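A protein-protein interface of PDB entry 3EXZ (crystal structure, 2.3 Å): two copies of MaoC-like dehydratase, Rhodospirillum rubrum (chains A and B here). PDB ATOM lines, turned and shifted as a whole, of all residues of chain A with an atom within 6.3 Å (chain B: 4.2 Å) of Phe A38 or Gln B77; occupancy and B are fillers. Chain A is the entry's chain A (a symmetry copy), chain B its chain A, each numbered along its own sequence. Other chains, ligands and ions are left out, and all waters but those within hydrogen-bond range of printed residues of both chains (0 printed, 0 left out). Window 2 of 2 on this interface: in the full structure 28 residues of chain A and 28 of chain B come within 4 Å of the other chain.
The backbone NH (N) of Ile B79 sits close to the side-chain amide nitrogen (NE2) of Gln A36 (2.6 Å).
The side-chain carboxylate (OD1) of Asp A34 lies close to the side-chain amide oxygen (OE1) of Gln A36, 3.0 Å away.
O of Phe A38 is in hydrogen-bond range of N of Ala A54 (3.4 Å).
Among the printed residues, merely in contact across the chains: Gln A36 with Gly B78, Leu A49 with Phe B143, Phe A38 with Ile B80 and Phe A38 with Gln B77.
Printed residues of chain B within 4 Å of Gln A36: Gly B78 (3.1 Å) and Ile B79 (2.6 Å).
Phe A38 touches just these residues of chain B: Gln B77 (3.9 Å) and Ile B80 (3.9 Å).
Of the printed residues of chain B, Leu A49 touches Phe B143 (3.7 Å).
Gly A52 touches none of the printed residues of chain B.
Of chain A, only Phe A38 (3.9 Å) comes within 4 Å of Gln B77.
Printed residues of chain A within 4 Å of Gly B78: Gln A36.
Printed residues of chain A within 4 Å of Ile B79: Gln A36 (2.6 Å).
Of the printed residues of chain A, Phe B143 touches Leu A49.
The nearest printed residue of chain B that does not touch Phe A38 is Ile B79 (4.2 Å).
The nearest residue of chain A that does not touch Gln B77 is Gln A36 (5.2 Å).
The nearest printed residue of chain B that does not touch Leu A49 is Ile B80 (4.3 Å).
Hydrophobic or aromatic side chains of chain A that line the printed part of chain B: Phe A38 and Leu A49.
Along chain A the printed residues that touch a printed residue of chain B span positions 36 to 49.
Hydrophobic or aromatic side chains of chain B that line the printed part of chain A: Ile B80 and Phe B143.
Among the printed residues, no Asp or Glu carboxylate lies within 4 Å of a Lys or Arg side-chain nitrogen of the other chain.
No position is printed for both chains.
Of the 5 pairs that touch across the chains among the printed residues, none has its exchanged pair printed and touching as well.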
ATOM      1  N   ILE A  26      20.776   5.758  17.409  1.00  0.00           N
ATOM      2  CA  ILE A  26      19.812   6.804  17.088  1.00  0.00           C
ATOM      3  C   ILE A  26      19.383   7.480  18.410  1.00  0.00           C
ATOM      4  O   ILE A  26      19.402   8.710  18.515  1.00  0.00           O
ATOM      5  CB  ILE A  26      18.592   6.205  16.357  1.00  0.00           C
ATOM      6  CG1 ILE A  26      19.033   5.759  14.957  1.00  0.00           C
ATOM      7  CG2 ILE A  26      17.460   7.213  16.309  1.00  0.00           C
ATOM      8  CD1 ILE A  26      17.956   5.073  14.129  1.00  0.00           C
ATOM      9  N   ASP A  34      18.960  15.893  19.877  1.00  0.00           N
ATOM     10  CA  ASP A  34      17.644  16.053  19.267  1.00  0.00           C
ATOM     11  C   ASP A  34      16.672  15.188  20.064  1.00  0.00           C
ATOM     12  O   ASP A  34      16.105  14.218  19.537  1.00  0.00           O
ATOM     13  CB  ASP A  34      17.669  15.581  17.809  1.00  0.00           C
ATOM     14  CG  ASP A  34      16.613  16.244  16.934  1.00  0.00           C
ATOM     15  OD1 ASP A  34      15.611  16.763  17.468  1.00  0.00           O
ATOM     16  OD2 ASP A  34      16.792  16.249  15.698  1.00  0.00           O
ATOM     17  N   GLN A  36      13.587  14.354  20.858  1.00  0.00           N
ATOM     18  CA  GLN A  36      12.187  14.392  20.488  1.00  0.00           C
ATOM     19  C   GLN A  36      11.693  12.957  20.437  1.00  0.00           C
ATOM     20  O   GLN A  36      12.412  12.056  19.999  1.00  0.00           O
ATOM     21  CB  GLN A  36      12.002  15.046  19.109  1.00  0.00           C
ATOM     22  CG  GLN A  36      12.566  16.445  19.025  1.00  0.00           C
ATOM     23  CD  GLN A  36      12.083  17.222  17.804  1.00  0.00           C
ATOM     24  OE1 GLN A  36      12.701  17.193  16.735  1.00  0.00           O
ATOM     25  NE2 GLN A  36      10.959  17.904  17.957  1.00  0.00           N
ATOM     26  N   PRO A  37      10.449  12.727  20.882  1.00  0.00           N
ATOM     27  CA  PRO A  37       9.823  11.400  20.912  1.00  0.00           C
ATOM     28  C   PRO A  37      10.098  10.524  19.700  1.00  0.00           C
ATOM     29  O   PRO A  37      10.493   9.364  19.852  1.00  0.00           O
ATOM     30  CB  PRO A  37       8.329  11.713  21.039  1.00  0.00           C
ATOM     31  CG  PRO A  37       8.310  13.009  21.769  1.00  0.00           C
ATOM     32  CD  PRO A  37       9.474  13.787  21.200  1.00  0.00           C
ATOM     33  N   PHE A  38       9.902  11.069  18.505  1.00  0.00           N
ATOM     34  CA  PHE A  38      10.107  10.262  17.315  1.00  0.00           C
ATOM     35  C   PHE A  38      11.520   9.741  17.071  1.00  0.00           C
ATOM     36  O   PHE A  38      11.716   8.851  16.237  1.00  0.00           O
ATOM     37  CB  PHE A  38       9.553  10.965  16.065  1.00  0.00           C
ATOM     38  CG  PHE A  38       9.572  12.456  16.131  1.00  0.00           C
ATOM     39  CD1 PHE A  38       8.454  13.163  16.557  1.00  0.00           C
ATOM     40  CD2 PHE A  38      10.680  13.160  15.689  1.00  0.00           C
ATOM     41  CE1 PHE A  38       8.441  14.553  16.529  1.00  0.00           C
ATOM     42  CE2 PHE A  38      10.674  14.546  15.660  1.00  0.00           C
ATOM     43  CZ  PHE A  38       9.551  15.242  16.080  1.00  0.00           C
ATOM     44  N   HIS A  39      12.495  10.258  17.813  1.00  0.00           N
ATOM     45  CA  HIS A  39      13.884   9.804  17.678  1.00  0.00           C
ATOM     46  C   HIS A  39      14.363   9.082  18.939  1.00  0.00           C
ATOM     47  O   HIS A  39      15.503   8.633  19.004  1.00  0.00           O
ATOM     48  CB  HIS A  39      14.803  11.006  17.443  1.00  0.00           C
ATOM     49  CG  HIS A  39      14.472  11.792  16.221  1.00  0.00           C
ATOM     50  ND1 HIS A  39      14.366  13.169  16.214  1.00  0.00           N
ATOM     51  CD2 HIS A  39      14.172  11.384  14.967  1.00  0.00           C
ATOM     52  CE1 HIS A  39      14.019  13.572  15.005  1.00  0.00           C
ATOM     53  NE2 HIS A  39      13.885  12.508  14.233  1.00  0.00           N
ATOM     54  N   LEU A  40      13.477   8.958  19.923  1.00  0.00           N
ATOM     55  CA  LEU A  40      13.804   8.368  21.218  1.00  0.00           C
ATOM     56  C   LEU A  40      13.019   7.135  21.605  1.00  0.00           C
ATOM     57  O   LEU A  40      13.516   6.270  22.331  1.00  0.00           O
ATOM     58  CB  LEU A  40      13.578   9.424  22.311  1.00  0.00           C
ATOM     59  CG  LEU A  40      14.603  10.552  22.413  1.00  0.00           C
ATOM     60  CD1 LEU A  40      14.179  11.587  23.463  1.00  0.00           C
ATOM     61  CD2 LEU A  40      15.950   9.931  22.768  1.00  0.00           C
ATOM     62  N   ASP A  41      11.782   7.065  21.135  1.00  0.00           N
ATOM     63  CA  ASP A  41      10.911   5.953  21.490  1.00  0.00           C
ATOM     64  C   ASP A  41      10.177   5.349  20.303  1.00  0.00           C
ATOM     65  O   ASP A  41       9.532   6.061  19.525  1.00  0.00           O
ATOM     66  CB  ASP A  41       9.901   6.412  22.554  1.00  0.00           C
ATOM     67  CG  ASP A  41       8.963   5.298  22.992  1.00  0.00           C
ATOM     68  OD1 ASP A  41       9.452   4.199  23.321  1.00  0.00           O
ATOM     69  OD2 ASP A  41       7.736   5.517  23.009  1.00  0.00           O
ATOM     70  N   ALA A  44       6.207   5.997  20.654  1.00  0.00           N
ATOM     71  CA  ALA A  44       5.879   7.392  20.376  1.00  0.00           C
ATOM     72  C   ALA A  44       6.124   7.706  18.884  1.00  0.00           C
ATOM     73  O   ALA A  44       5.381   8.481  18.286  1.00  0.00           O
ATOM     74  CB  ALA A  44       6.737   8.309  21.238  1.00  0.00           C
ATOM     75  N   ALA A  45       7.149   7.098  18.280  1.00  0.00           N
ATOM     76  CA  ALA A  45       7.465   7.356  16.870  1.00  0.00           C
ATOM     77  C   ALA A  45       6.381   6.828  15.931  1.00  0.00           C
ATOM     78  O   ALA A  45       6.076   7.442  14.904  1.00  0.00           O
ATOM     79  CB  ALA A  45       8.817   6.755  16.522  1.00  0.00           C
ATOM     80  N   SER A  48       3.758   9.277  15.049  1.00  0.00           N
ATOM     81  CA  SER A  48       4.245  10.533  14.477  1.00  0.00           C
ATOM     82  C   SER A  48       4.229  10.450  12.953  1.00  0.00           C
ATOM     83  O   SER A  48       3.858   9.425  12.383  1.00  0.00           O
ATOM     84  CB  SER A  48       5.687  10.793  14.921  1.00  0.00           C
ATOM     85  OG  SER A  48       6.574   9.828  14.370  1.00  0.00           O
ATOM     86  N   LEU A  49       4.627  11.540  12.299  1.00  0.00           N
ATOM     87  CA  LEU A  49       4.701  11.574  10.839  1.00  0.00           C
ATOM     88  C   LEU A  49       5.679  10.507  10.334  1.00  0.00           C
ATOM     89  O   LEU A  49       5.494   9.944   9.252  1.00  0.00           O
ATOM     90  CB  LEU A  49       5.180  12.944  10.339  1.00  0.00           C
ATOM     91  CG  LEU A  49       4.138  14.063  10.229  1.00  0.00           C
ATOM     92  CD1 LEU A  49       4.638  15.132   9.254  1.00  0.00           C
ATOM     93  CD2 LEU A  49       2.807  13.485   9.739  1.00  0.00           C
ATOM     94  N   PHE A  50       6.725  10.246  11.117  1.00  0.00           N
ATOM     95  CA  PHE A  50       7.740   9.254  10.770  1.00  0.00           C
ATOM     96  C   PHE A  50       7.154   7.844  10.851  1.00  0.00           C
ATOM     97  O   PHE A  50       7.656   6.920  10.211  1.00  0.00           O
ATOM     98  CB  PHE A  50       8.937   9.360  11.735  1.00  0.00           C
ATOM     99  CG  PHE A  50       9.691  10.662  11.640  1.00  0.00           C
ATOM    100  CD1 PHE A  50      10.685  10.842  10.682  1.00  0.00           C
ATOM    101  CD2 PHE A  50       9.382  11.724  12.490  1.00  0.00           C
ATOM    102  CE1 PHE A  50      11.360  12.064  10.568  1.00  0.00           C
ATOM    103  CE2 PHE A  50      10.049  12.945  12.386  1.00  0.00           C
ATOM    104  CZ  PHE A  50      11.040  13.115  11.421  1.00  0.00           C
ATOM    105  N   GLY A  52       7.249   5.433  13.152  1.00  0.00           N
ATOM    106  CA  GLY A  52       8.315   4.493  13.466  1.00  0.00           C
ATOM    107  C   GLY A  52       9.614   5.236  13.772  1.00  0.00           C
ATOM    108  O   GLY A  52       9.795   6.389  13.372  1.00  0.00           O
ATOM    109  N   LEU A  53      10.522   4.584  14.486  1.00  0.00           N
ATOM    110  CA  LEU A  53      11.783   5.216  14.830  1.00  0.00           C
ATOM    111  C   LEU A  53      12.490   5.745  13.590  1.00  0.00           C
ATOM    112  O   LEU A  53      12.581   5.057  12.573  1.00  0.00           O
ATOM    113  CB  LEU A  53      12.726   4.221  15.535  1.00  0.00           C
ATOM    114  CG  LEU A  53      13.345   4.570  16.906  1.00  0.00           C
ATOM    115  CD1 LEU A  53      14.797   4.078  16.945  1.00  0.00           C
ATOM    116  CD2 LEU A  53      13.276   6.070  17.168  1.00  0.00           C
ATOM    117  N   ALA A  54      12.944   6.988  13.661  1.00  0.00           N
ATOM    118  CA  ALA A  54      13.727   7.565  12.581  1.00  0.00           C
ATOM    119  C   ALA A  54      14.876   8.299  13.262  1.00  0.00           C
ATOM    120  O   ALA A  54      14.778   8.697  14.430  1.00  0.00           O
ATOM    121  CB  ALA A  54      12.915   8.519  11.731  1.00  0.00           C
ATOM    122  N   ALA A  55      15.990   8.436  12.560  1.00  0.00           N
ATOM    123  CA  ALA A  55      17.123   9.143  13.121  1.00  0.00           C
ATOM    124  C   ALA A  55      16.921  10.643  12.897  1.00  0.00           C
ATOM    125  O   ALA A  55      16.192  11.065  11.994  1.00  0.00           O
ATOM    126  CB  ALA A  55      18.425   8.676  12.441  1.00  0.00           C
ATOM    127  N   PHE B   4       1.284  25.936  18.322  1.00  0.00           N
ATOM    128  CA  PHE B   4       0.802  25.231  17.140  1.00  0.00           C
ATOM    129  C   PHE B   4       0.786  26.285  16.017  1.00  0.00           C
ATOM    130  O   PHE B   4       1.119  27.454  16.243  1.00  0.00           O
ATOM    131  CB  PHE B   4      -0.598  24.650  17.329  1.00  0.00           C
ATOM    132  CG  PHE B   4      -0.676  23.588  18.387  1.00  0.00           C
ATOM    133  CD1 PHE B   4      -0.515  22.242  18.066  1.00  0.00           C
ATOM    134  CD2 PHE B   4      -0.972  23.933  19.703  1.00  0.00           C
ATOM    135  CE1 PHE B   4      -0.648  21.254  19.045  1.00  0.00           C
ATOM    136  CE2 PHE B   4      -1.107  22.953  20.688  1.00  0.00           C
ATOM    137  CZ  PHE B   4      -0.952  21.612  20.355  1.00  0.00           C
ATOM    138  N   LEU B  75       7.697  24.430  19.695  1.00  0.00           N
ATOM    139  CA  LEU B  75       6.616  23.774  18.974  1.00  0.00           C
ATOM    140  C   LEU B  75       6.044  22.604  19.759  1.00  0.00           C
ATOM    141  O   LEU B  75       6.784  21.717  20.185  1.00  0.00           O
ATOM    142  CB  LEU B  75       7.125  23.311  17.609  1.00  0.00           C
ATOM    143  CG  LEU B  75       6.938  24.194  16.357  1.00  0.00           C
ATOM    144  CD1 LEU B  75       6.694  25.663  16.704  1.00  0.00           C
ATOM    145  CD2 LEU B  75       8.165  24.027  15.471  1.00  0.00           C
ATOM    146  N   ALA B  76       4.725  22.590  19.932  1.00  0.00           N
ATOM    147  CA  ALA B  76       4.079  21.536  20.708  1.00  0.00           C
ATOM    148  C   ALA B  76       4.234  20.141  20.128  1.00  0.00           C
ATOM    149  O   ALA B  76       4.405  19.167  20.870  1.00  0.00           O
ATOM    150  CB  ALA B  76       2.594  21.864  20.905  1.00  0.00           C
ATOM    151  N   GLN B  77       4.192  20.047  18.803  1.00  0.00           N
ATOM    152  CA  GLN B  77       4.320  18.757  18.148  1.00  0.00           C
ATOM    153  C   GLN B  77       5.727  18.435  17.645  1.00  0.00           C
ATOM    154  O   GLN B  77       5.924  17.505  16.858  1.00  0.00           O
ATOM    155  CB  GLN B  77       3.282  18.634  17.028  1.00  0.00           C
ATOM    156  CG  GLN B  77       1.845  18.779  17.516  1.00  0.00           C
ATOM    157  CD  GLN B  77       0.841  18.529  16.411  1.00  0.00           C
ATOM    158  OE1 GLN B  77       0.831  19.227  15.399  1.00  0.00           O
ATOM    159  NE2 GLN B  77      -0.007  17.525  16.596  1.00  0.00           N
ATOM    160  N   GLY B  78       6.703  19.209  18.105  1.00  0.00           N
ATOM    161  CA  GLY B  78       8.077  18.942  17.729  1.00  0.00           C
ATOM    162  C   GLY B  78       8.582  19.705  16.535  1.00  0.00           C
ATOM    163  O   GLY B  78       7.834  20.455  15.909  1.00  0.00           O
ATOM    164  N   ILE B  79       9.851  19.508  16.198  1.00  0.00           N
ATOM    165  CA  ILE B  79      10.436  20.211  15.066  1.00  0.00           C
ATOM    166  C   ILE B  79      10.769  19.194  13.990  1.00  0.00           C
ATOM    167  O   ILE B  79      11.610  18.319  14.182  1.00  0.00           O
ATOM    168  CB  ILE B  79      11.697  21.002  15.497  1.00  0.00           C
ATOM    169  CG1 ILE B  79      11.315  22.027  16.584  1.00  0.00           C
ATOM    170  CG2 ILE B  79      12.311  21.707  14.277  1.00  0.00           C
ATOM    171  CD1 ILE B  79      12.502  22.661  17.280  1.00  0.00           C
ATOM    172  N   ILE B  80      10.086  19.304  12.859  1.00  0.00           N
ATOM    173  CA  ILE B  80      10.297  18.384  11.755  1.00  0.00           C
ATOM    174  C   ILE B  80      10.802  19.171  10.558  1.00  0.00           C
ATOM    175  O   ILE B  80      10.073  19.961   9.949  1.00  0.00           O
ATOM    176  CB  ILE B  80       8.994  17.621  11.443  1.00  0.00           C
ATOM    177  CG1 ILE B  80       8.640  16.709  12.629  1.00  0.00           C
ATOM    178  CG2 ILE B  80       9.167  16.781  10.194  1.00  0.00           C
ATOM    179  CD1 ILE B  80       7.308  15.991  12.469  1.00  0.00           C
ATOM    180  N   PHE B 143       1.735  21.744  12.048  1.00  0.00           N
ATOM    181  CA  PHE B 143       0.300  21.486  11.993  1.00  0.00           C
ATOM    182  C   PHE B 143      -0.450  22.375  13.002  1.00  0.00           C
ATOM    183  O   PHE B 143       0.130  22.853  13.981  1.00  0.00           O
ATOM    184  CB  PHE B 143       0.011  20.024  12.364  1.00  0.00           C
ATOM    185  CG  PHE B 143       0.494  19.031  11.351  1.00  0.00           C
ATOM    186  CD1 PHE B 143      -0.392  18.455  10.447  1.00  0.00           C
ATOM    187  CD2 PHE B 143       1.830  18.655  11.308  1.00  0.00           C
ATOM    188  CE1 PHE B 143       0.054  17.533   9.498  1.00  0.00           C
ATOM    189  CE2 PHE B 143       2.285  17.736  10.363  1.00  0.00           C
ATOM    190  CZ  PHE B 143       1.394  17.168   9.465  1.00  0.00           C
ATOM    191  N   PRO B 146      -4.779  19.885  17.028  1.00  0.00           N
ATOM    192  CA  PRO B 146      -5.828  18.915  16.711  1.00  0.00           C
ATOM    193  C   PRO B 146      -7.137  19.306  17.384  1.00  0.00           C
ATOM    194  O   PRO B 146      -7.145  20.100  18.327  1.00  0.00           O
ATOM    195  CB  PRO B 146      -5.296  17.610  17.306  1.00  0.00           C
ATOM    196  CG  PRO B 146      -3.826  17.792  17.346  1.00  0.00           C
ATOM    197  CD  PRO B 146      -3.640  19.238  17.703  1.00  0.00           C
